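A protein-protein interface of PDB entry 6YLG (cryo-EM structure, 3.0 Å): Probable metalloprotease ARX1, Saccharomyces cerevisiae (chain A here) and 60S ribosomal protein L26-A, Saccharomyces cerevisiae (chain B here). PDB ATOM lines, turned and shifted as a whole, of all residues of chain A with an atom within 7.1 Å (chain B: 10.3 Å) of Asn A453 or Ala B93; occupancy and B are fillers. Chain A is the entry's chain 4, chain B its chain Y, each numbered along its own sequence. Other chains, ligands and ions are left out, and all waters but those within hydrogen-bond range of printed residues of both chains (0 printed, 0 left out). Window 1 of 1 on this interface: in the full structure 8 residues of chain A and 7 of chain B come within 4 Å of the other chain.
The side-chain amino group (NZ) of Lys B89 lies within hydrogen-bond range of the backbone carbonyl oxygen (O) of Pro A454 (3.1 Å).
The backbone carbonyl oxygen (O) of Asn B91 sits at hydrogen-bond distance from the side-chain amide nitrogen (ND2) of Asn A457.
The backbone carbonyl oxygen of Gly B92 lies within hydrogen-bond range of the side-chain amide nitrogen of Asn A453 (3.0 Å).
The backbone carbonyl oxygen (O) of Ser B94 is in hydrogen-bond range of the side-chain hydroxyl (OG1) of Thr A452 (3.0 Å).
The side-chain hydroxyl (OG) of Ser B94 lies within hydrogen-bond range of the side-chain amide oxygen (OD1) of Asn A453 (3.1 Å).
The backbone NH of Lys B87 sits at hydrogen-bond distance from the backbone carbonyl oxygen of Val B95 (3.1 Å).
ND2 of Asn A453 is in hydrogen-bond range of O of Leu A478 (3.4 Å).
The backbone carbonyl oxygen (O) of Gly A479 is in hydrogen-bond range of the side-chain amide nitrogen (ND2) of Asn A453 (3.3 Å).
The backbone carbonyl oxygen (O) of Asn A455 lies within hydrogen-bond range of the side-chain hydroxyl (OG) of Ser A459, 2.8 Å away.
Ser B94 touches Ala A451.
Ala B93 touches Asn A453.
O of Pro A454 touches CB of Ala B93, 3.5 Å away.
N of Pro A454 touches O of Ser B94 (3.7 Å).
CA of Pro A454 touches CG1 of Val B95 (3.9 Å).
Lys B89 touches Asn A455 (NZ to OD1, 3.7 Å).
N of Asn A455 touches CB of Ala B93 (3.7 Å).
Gly A456 touches Asn B91.
Gly A456 touches Ala B93.
Gly B92 touches Leu A478.
Of the printed residues of chain B, Asn A453 touches Gly B92, Ala B93 and Ser B94.
Ala B93 touches just these residues of chain A: Asn A453, Pro A454, Asn A455 and Gly A456.
Of chain B, only Ser B94 (3.0 Å) and Pro B96 (3.6 Å) come within 4 Å of Thr A452.
Printed residues of chain B within 4 Å of Pro A454: Lys B89, Ala B93, Ser B94 and Val B95.
Printed residues of chain B within 4 Å of Gly A456: Asn B91 and Ala B93.
No residue of chain B comes within 4 Å of Gly A479.
Of the printed residues of chain B, Ala A451 touches Ser B94.
Printed residues of chain B within 4 Å of Leu A478: Gly B92 (3.5 Å).
Printed residues of chain B within 4 Å of Asn A455: Lys B89 and Ala B93.
Printed residues of chain A within 4 Å of Lys B89: Pro A454 (3.1 Å) and Asn A455 (3.7 Å).
Of the printed residues of chain A, Asn B91 touches Gly A456 (3.5 Å) and Asn A457 (3.1 Å).
Val A480 touches none of the printed residues of chain B.
Val B90 touches none of the printed residues of chain A.
The nearest residue of chain B that does not touch Asn A453 is Val B95 (5.4 Å).
The nearest residue of chain A that does not touch Ala B93 is Gly A479 (5.5 Å).
Of the 14 printed residues of chain B, 7 touch a printed residue of chain A.
Printed residues of chain B that touch a printed residue of chain A: Lys B89, Asn B91, Gly B92, Ala B93, Ser B94, Val B95 and Pro B96.
Among the printed residues, no Asp or Glu carboxylate lies within 4 Å of a Lys or Arg side-chain nitrogen of the other chain.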
ATOM      1  N   ILE A 448     -23.519   7.316  24.120  1.00  0.00           N
ATOM      2  CA  ILE A 448     -23.208   5.910  23.888  1.00  0.00           C
ATOM      3  C   ILE A 448     -22.898   5.210  25.203  1.00  0.00           C
ATOM      4  O   ILE A 448     -23.342   4.080  25.441  1.00  0.00           O
ATOM      5  CB  ILE A 448     -22.043   5.788  22.888  1.00  0.00           C
ATOM      6  CG1 ILE A 448     -22.484   6.252  21.496  1.00  0.00           C
ATOM      7  CG2 ILE A 448     -21.512   4.357  22.835  1.00  0.00           C
ATOM      8  CD1 ILE A 448     -21.482   7.148  20.816  1.00  0.00           C
ATOM      9  N   ALA A 451     -25.866   4.767  27.312  1.00  0.00           N
ATOM     10  CA  ALA A 451     -26.916   4.046  26.613  1.00  0.00           C
ATOM     11  C   ALA A 451     -27.289   2.764  27.350  1.00  0.00           C
ATOM     12  O   ALA A 451     -26.661   2.363  28.335  1.00  0.00           O
ATOM     13  CB  ALA A 451     -26.474   3.707  25.192  1.00  0.00           C
ATOM     14  N   THR A 452     -28.340   2.119  26.847  1.00  0.00           N
ATOM     15  CA  THR A 452     -28.788   0.816  27.334  1.00  0.00           C
ATOM     16  C   THR A 452     -29.101  -0.053  26.123  1.00  0.00           C
ATOM     17  O   THR A 452     -30.027   0.247  25.363  1.00  0.00           O
ATOM     18  CB  THR A 452     -30.006   0.947  28.250  1.00  0.00           C
ATOM     19  OG1 THR A 452     -30.596  -0.344  28.457  1.00  0.00           O
ATOM     20  CG2 THR A 452     -31.041   1.899  27.665  1.00  0.00           C
ATOM     21  N   ASN A 453     -28.330  -1.123  25.949  1.00  0.00           N
ATOM     22  CA  ASN A 453     -28.501  -2.078  24.858  1.00  0.00           C
ATOM     23  C   ASN A 453     -28.800  -3.465  25.428  1.00  0.00           C
ATOM     24  O   ASN A 453     -27.872  -4.234  25.691  1.00  0.00           O
ATOM     25  CB  ASN A 453     -27.253  -2.140  23.977  1.00  0.00           C
ATOM     26  CG  ASN A 453     -25.964  -2.088  24.769  1.00  0.00           C
ATOM     27  OD1 ASN A 453     -25.860  -1.368  25.762  1.00  0.00           O
ATOM     28  ND2 ASN A 453     -24.969  -2.844  24.326  1.00  0.00           N
ATOM     29  N   PRO A 454     -30.068  -3.832  25.641  1.00  0.00           N
ATOM     30  CA  PRO A 454     -30.380  -5.079  26.354  1.00  0.00           C
ATOM     31  C   PRO A 454     -29.872  -6.357  25.703  1.00  0.00           C
ATOM     32  O   PRO A 454     -29.939  -7.411  26.341  1.00  0.00           O
ATOM     33  CB  PRO A 454     -31.916  -5.072  26.389  1.00  0.00           C
ATOM     34  CG  PRO A 454     -32.284  -3.661  26.320  1.00  0.00           C
ATOM     35  CD  PRO A 454     -31.287  -3.036  25.407  1.00  0.00           C
ATOM     36  N   ASN A 455     -29.374  -6.315  24.469  1.00  0.00           N
ATOM     37  CA  ASN A 455     -28.726  -7.480  23.871  1.00  0.00           C
ATOM     38  C   ASN A 455     -27.649  -6.974  22.925  1.00  0.00           C
ATOM     39  O   ASN A 455     -27.958  -6.306  21.933  1.00  0.00           O
ATOM     40  CB  ASN A 455     -29.733  -8.367  23.138  1.00  0.00           C
ATOM     41  CG  ASN A 455     -30.170  -9.584  23.954  1.00  0.00           C
ATOM     42  OD1 ASN A 455     -29.742  -9.791  25.090  1.00  0.00           O
ATOM     43  ND2 ASN A 455     -31.024 -10.404  23.358  1.00  0.00           N
ATOM     44  N   GLY A 456     -26.399  -7.294  23.236  1.00  0.00           N
ATOM     45  CA  GLY A 456     -25.248  -6.852  22.464  1.00  0.00           C
ATOM     46  C   GLY A 456     -24.637  -8.023  21.717  1.00  0.00           C
ATOM     47  O   GLY A 456     -24.634  -9.151  22.215  1.00  0.00           O
ATOM     48  N   ASN A 457     -24.155  -7.741  20.502  1.00  0.00           N
ATOM     49  CA  ASN A 457     -23.570  -8.718  19.586  1.00  0.00           C
ATOM     50  C   ASN A 457     -24.616  -9.627  18.943  1.00  0.00           C
ATOM     51  O   ASN A 457     -24.268 -10.455  18.095  1.00  0.00           O
ATOM     52  CB  ASN A 457     -22.510  -9.581  20.284  1.00  0.00           C
ATOM     53  CG  ASN A 457     -21.547  -8.765  21.117  1.00  0.00           C
ATOM     54  OD1 ASN A 457     -21.537  -7.538  21.052  1.00  0.00           O
ATOM     55  ND2 ASN A 457     -20.731  -9.446  21.909  1.00  0.00           N
ATOM     56  N   SER A 459     -27.960  -8.181  18.109  1.00  0.00           N
ATOM     57  CA  SER A 459     -28.930  -7.349  17.416  1.00  0.00           C
ATOM     58  C   SER A 459     -28.587  -7.282  15.933  1.00  0.00           C
ATOM     59  O   SER A 459     -27.604  -6.641  15.547  1.00  0.00           O
ATOM     60  CB  SER A 459     -28.956  -5.947  18.019  1.00  0.00           C
ATOM     61  OG  SER A 459     -29.188  -5.994  19.414  1.00  0.00           O
ATOM     62  N   LEU A 478     -18.024  -2.616  23.831  1.00  0.00           N
ATOM     63  CA  LEU A 478     -19.289  -1.979  24.205  1.00  0.00           C
ATOM     64  C   LEU A 478     -20.508  -2.680  23.608  1.00  0.00           C
ATOM     65  O   LEU A 478     -21.643  -2.338  23.955  1.00  0.00           O
ATOM     66  CB  LEU A 478     -19.328  -0.501  23.800  1.00  0.00           C
ATOM     67  CG  LEU A 478     -18.095   0.367  24.033  1.00  0.00           C
ATOM     68  CD1 LEU A 478     -18.488   1.817  23.844  1.00  0.00           C
ATOM     69  CD2 LEU A 478     -17.499   0.132  25.411  1.00  0.00           C
ATOM     70  N   GLY A 479     -20.299  -3.661  22.735  1.00  0.00           N
ATOM     71  CA  GLY A 479     -21.363  -4.546  22.297  1.00  0.00           C
ATOM     72  C   GLY A 479     -22.569  -3.899  21.648  1.00  0.00           C
ATOM     73  O   GLY A 479     -23.672  -4.452  21.732  1.00  0.00           O
ATOM     74  N   VAL A 480     -22.394  -2.744  21.004  1.00  0.00           N
ATOM     75  CA  VAL A 480     -23.414  -1.964  20.311  1.00  0.00           C
ATOM     76  C   VAL A 480     -23.340  -2.270  18.822  1.00  0.00           C
ATOM     77  O   VAL A 480     -22.257  -2.513  18.275  1.00  0.00           O
ATOM     78  CB  VAL A 480     -23.249  -0.456  20.593  1.00  0.00           C
ATOM     79  CG1 VAL A 480     -22.970  -0.220  22.069  1.00  0.00           C
ATOM     80  CG2 VAL A 480     -22.152   0.164  19.746  1.00  0.00           C
ATOM     81  N   SER A 481     -24.472  -2.364  18.132  1.00  0.00           N
ATOM     82  CA  SER A 481     -24.466  -2.587  16.694  1.00  0.00           C
ATOM     83  C   SER A 481     -24.949  -1.348  15.953  1.00  0.00           C
ATOM     84  O   SER A 481     -25.306  -0.331  16.553  1.00  0.00           O
ATOM     85  CB  SER A 481     -25.348  -3.780  16.328  1.00  0.00           C
ATOM     86  OG  SER A 481     -25.215  -4.095  14.955  1.00  0.00           O
ATOM     87  N   LYS A 484     -28.603  -0.043  17.010  1.00  0.00           N
ATOM     88  CA  LYS A 484     -28.675   0.757  18.227  1.00  0.00           C
ATOM     89  C   LYS A 484     -27.868   2.040  18.081  1.00  0.00           C
ATOM     90  O   LYS A 484     -28.195   3.060  18.696  1.00  0.00           O
ATOM     91  CB  LYS A 484     -28.189  -0.064  19.424  1.00  0.00           C
ATOM     92  CG  LYS A 484     -28.083   0.691  20.758  1.00  0.00           C
ATOM     93  CD  LYS A 484     -29.393   1.360  21.186  1.00  0.00           C
ATOM     94  CE  LYS A 484     -29.202   2.224  22.419  1.00  0.00           C
ATOM     95  NZ  LYS A 484     -29.996   1.748  23.576  1.00  0.00           N
ATOM     96  N   LEU A 488     -29.261   5.744  18.745  1.00  0.00           N
ATOM     97  CA  LEU A 488     -28.623   6.749  19.589  1.00  0.00           C
ATOM     98  C   LEU A 488     -28.315   8.023  18.816  1.00  0.00           C
ATOM     99  O   LEU A 488     -28.448   9.126  19.357  1.00  0.00           O
ATOM    100  CB  LEU A 488     -27.341   6.182  20.187  1.00  0.00           C
ATOM    101  CG  LEU A 488     -27.544   5.097  21.241  1.00  0.00           C
ATOM    102  CD1 LEU A 488     -26.223   4.428  21.574  1.00  0.00           C
ATOM    103  CD2 LEU A 488     -28.202   5.671  22.494  1.00  0.00           C
ATOM    104  N   GLN B  81     -35.718   4.542  35.866  1.00  0.00           N
ATOM    105  CA  GLN B  81     -34.490   3.997  35.304  1.00  0.00           C
ATOM    106  C   GLN B  81     -33.419   5.076  35.370  1.00  0.00           C
ATOM    107  O   GLN B  81     -33.526   6.111  34.702  1.00  0.00           O
ATOM    108  CB  GLN B  81     -34.715   3.526  33.872  1.00  0.00           C
ATOM    109  CG  GLN B  81     -35.742   2.428  33.749  1.00  0.00           C
ATOM    110  CD  GLN B  81     -35.731   1.778  32.385  1.00  0.00           C
ATOM    111  OE1 GLN B  81     -35.214   2.342  31.422  1.00  0.00           O
ATOM    112  NE2 GLN B  81     -36.298   0.583  32.295  1.00  0.00           N
ATOM    113  N   VAL B  85     -26.494   2.684  36.765  1.00  0.00           N
ATOM    114  CA  VAL B  85     -26.929   1.519  37.532  1.00  0.00           C
ATOM    115  C   VAL B  85     -27.503   0.509  36.549  1.00  0.00           C
ATOM    116  O   VAL B  85     -28.651   0.627  36.109  1.00  0.00           O
ATOM    117  CB  VAL B  85     -27.944   1.892  38.629  1.00  0.00           C
ATOM    118  CG1 VAL B  85     -27.230   2.454  39.835  1.00  0.00           C
ATOM    119  CG2 VAL B  85     -28.942   2.898  38.132  1.00  0.00           C
ATOM    120  N   THR B  86     -26.703  -0.491  36.198  1.00  0.00           N
ATOM    121  CA  THR B  86     -27.044  -1.415  35.130  1.00  0.00           C
ATOM    122  C   THR B  86     -26.476  -2.787  35.444  1.00  0.00           C
ATOM    123  O   THR B  86     -25.413  -2.914  36.057  1.00  0.00           O
ATOM    124  CB  THR B  86     -26.504  -0.935  33.777  1.00  0.00           C
ATOM    125  OG1 THR B  86     -25.200  -0.366  33.952  1.00  0.00           O
ATOM    126  CG2 THR B  86     -27.428   0.105  33.168  1.00  0.00           C
ATOM    127  N   LYS B  87     -27.206  -3.812  35.021  1.00  0.00           N
ATOM    128  CA  LYS B  87     -26.744  -5.194  35.089  1.00  0.00           C
ATOM    129  C   LYS B  87     -26.063  -5.495  33.760  1.00  0.00           C
ATOM    130  O   LYS B  87     -26.727  -5.704  32.742  1.00  0.00           O
ATOM    131  CB  LYS B  87     -27.898  -6.151  35.361  1.00  0.00           C
ATOM    132  CG  LYS B  87     -27.432  -7.506  35.858  1.00  0.00           C
ATOM    133  CD  LYS B  87     -28.411  -8.618  35.544  1.00  0.00           C
ATOM    134  CE  LYS B  87     -27.712  -9.958  35.577  1.00  0.00           C
ATOM    135  NZ  LYS B  87     -26.992 -10.191  36.853  1.00  0.00           N
ATOM    136  N   GLU B  88     -24.734  -5.513  33.776  1.00  0.00           N
ATOM    137  CA  GLU B  88     -23.959  -5.679  32.556  1.00  0.00           C
ATOM    138  C   GLU B  88     -23.719  -7.160  32.301  1.00  0.00           C
ATOM    139  O   GLU B  88     -23.123  -7.852  33.133  1.00  0.00           O
ATOM    140  CB  GLU B  88     -22.633  -4.932  32.662  1.00  0.00           C
ATOM    141  CG  GLU B  88     -22.648  -3.541  32.045  1.00  0.00           C
ATOM    142  CD  GLU B  88     -23.418  -2.530  32.874  1.00  0.00           C
ATOM    143  OE1 GLU B  88     -23.448  -2.663  34.115  1.00  0.00           O
ATOM    144  OE2 GLU B  88     -23.992  -1.594  32.280  1.00  0.00           O
ATOM    145  N   LYS B  89     -24.187  -7.643  31.154  1.00  0.00           N
ATOM    146  CA  LYS B  89     -23.919  -9.014  30.752  1.00  0.00           C
ATOM    147  C   LYS B  89     -22.558  -9.102  30.067  1.00  0.00           C
ATOM    148  O   LYS B  89     -21.964  -8.098  29.665  1.00  0.00           O
ATOM    149  CB  LYS B  89     -25.019  -9.527  29.826  1.00  0.00           C
ATOM    150  CG  LYS B  89     -26.191 -10.143  30.564  1.00  0.00           C
ATOM    151  CD  LYS B  89     -27.379 -10.364  29.649  1.00  0.00           C
ATOM    152  CE  LYS B  89     -28.257  -9.130  29.558  1.00  0.00           C
ATOM    153  NZ  LYS B  89     -29.462  -9.387  28.731  1.00  0.00           N
ATOM    154  N   VAL B  90     -22.063 -10.335  29.939  1.00  0.00           N
ATOM    155  CA  VAL B  90     -20.696 -10.535  29.469  1.00  0.00           C
ATOM    156  C   VAL B  90     -20.552 -10.149  28.003  1.00  0.00           C
ATOM    157  O   VAL B  90     -19.465  -9.752  27.567  1.00  0.00           O
ATOM    158  CB  VAL B  90     -20.263 -11.993  29.717  1.00  0.00           C
ATOM    159  CG1 VAL B  90     -20.931 -12.934  28.722  1.00  0.00           C
ATOM    160  CG2 VAL B  90     -18.748 -12.115  29.650  1.00  0.00           C
ATOM    161  N   ASN B  91     -21.626 -10.260  27.218  1.00  0.00           N
ATOM    162  CA  ASN B  91     -21.538  -9.909  25.805  1.00  0.00           C
ATOM    163  C   ASN B  91     -21.251  -8.427  25.609  1.00  0.00           C
ATOM    164  O   ASN B  91     -20.531  -8.051  24.678  1.00  0.00           O
ATOM    165  CB  ASN B  91     -22.830 -10.297  25.079  1.00  0.00           C
ATOM    166  CG  ASN B  91     -24.068  -9.619  25.657  1.00  0.00           C
ATOM    167  OD1 ASN B  91     -24.140  -8.395  25.758  1.00  0.00           O
ATOM    168  ND2 ASN B  91     -25.056 -10.422  26.024  1.00  0.00           N
ATOM    169  N   GLY B  92     -21.796  -7.583  26.479  1.00  0.00           N
ATOM    170  CA  GLY B  92     -21.793  -6.141  26.303  1.00  0.00           C
ATOM    171  C   GLY B  92     -23.142  -5.501  26.532  1.00  0.00           C
ATOM    172  O   GLY B  92     -23.258  -4.275  26.400  1.00  0.00           O
ATOM    173  N   ALA B  93     -24.169  -6.277  26.871  1.00  0.00           N
ATOM    174  CA  ALA B  93     -25.503  -5.729  27.054  1.00  0.00           C
ATOM    175  C   ALA B  93     -25.656  -5.144  28.448  1.00  0.00           C
ATOM    176  O   ALA B  93     -25.188  -5.725  29.432  1.00  0.00           O
ATOM    177  CB  ALA B  93     -26.553  -6.810  26.829  1.00  0.00           C
ATOM    178  N   SER B  94     -26.311  -3.992  28.524  1.00  0.00           N
ATOM    179  CA  SER B  94     -26.653  -3.350  29.784  1.00  0.00           C
ATOM    180  C   SER B  94     -28.156  -3.128  29.829  1.00  0.00           C
ATOM    181  O   SER B  94     -28.736  -2.598  28.876  1.00  0.00           O
ATOM    182  CB  SER B  94     -25.918  -2.019  29.938  1.00  0.00           C
ATOM    183  OG  SER B  94     -26.223  -1.143  28.868  1.00  0.00           O
ATOM    184  N   VAL B  95     -28.776  -3.538  30.930  1.00  0.00           N
ATOM    185  CA  VAL B  95     -30.195  -3.336  31.182  1.00  0.00           C
ATOM    186  C   VAL B  95     -30.307  -2.454  32.420  1.00  0.00           C
ATOM    187  O   VAL B  95     -29.516  -2.609  33.355  1.00  0.00           O
ATOM    188  CB  VAL B  95     -30.951  -4.660  31.387  1.00  0.00           C
ATOM    189  CG1 VAL B  95     -30.732  -5.582  30.209  1.00  0.00           C
ATOM    190  CG2 VAL B  95     -30.532  -5.341  32.683  1.00  0.00           C
ATOM    191  N   PRO B  96     -31.252  -1.514  32.493  1.00  0.00           N
ATOM    192  CA  PRO B  96     -31.327  -0.675  33.690  1.00  0.00           C
ATOM    193  C   PRO B  96     -31.978  -1.422  34.841  1.00  0.00           C
ATOM    194  O   PRO B  96     -32.867  -2.254  34.649  1.00  0.00           O
ATOM    195  CB  PRO B  96     -32.181   0.519  33.244  1.00  0.00           C
ATOM    196  CG  PRO B  96     -32.424   0.321  31.775  1.00  0.00           C
ATOM    197  CD  PRO B  96     -32.316  -1.137  31.548  1.00  0.00           C
ATOM    198  N   ILE B  97     -31.522  -1.117  36.046  1.00  0.00           N
ATOM    199  CA  ILE B  97     -32.129  -1.640  37.260  1.00  0.00           C
ATOM    200  C   ILE B  97     -33.356  -0.789  37.552  1.00  0.00           C
ATOM    201  O   ILE B  97     -33.287   0.446  37.519  1.00  0.00           O
ATOM    202  CB  ILE B  97     -31.127  -1.625  38.430  1.00  0.00           C
ATOM    203  CG1 ILE B  97     -30.239  -2.875  38.393  1.00  0.00           C
ATOM    204  CG2 ILE B  97     -31.832  -1.545  39.789  1.00  0.00           C
ATOM    205  CD1 ILE B  97     -29.269  -2.914  37.242  1.00  0.00           C
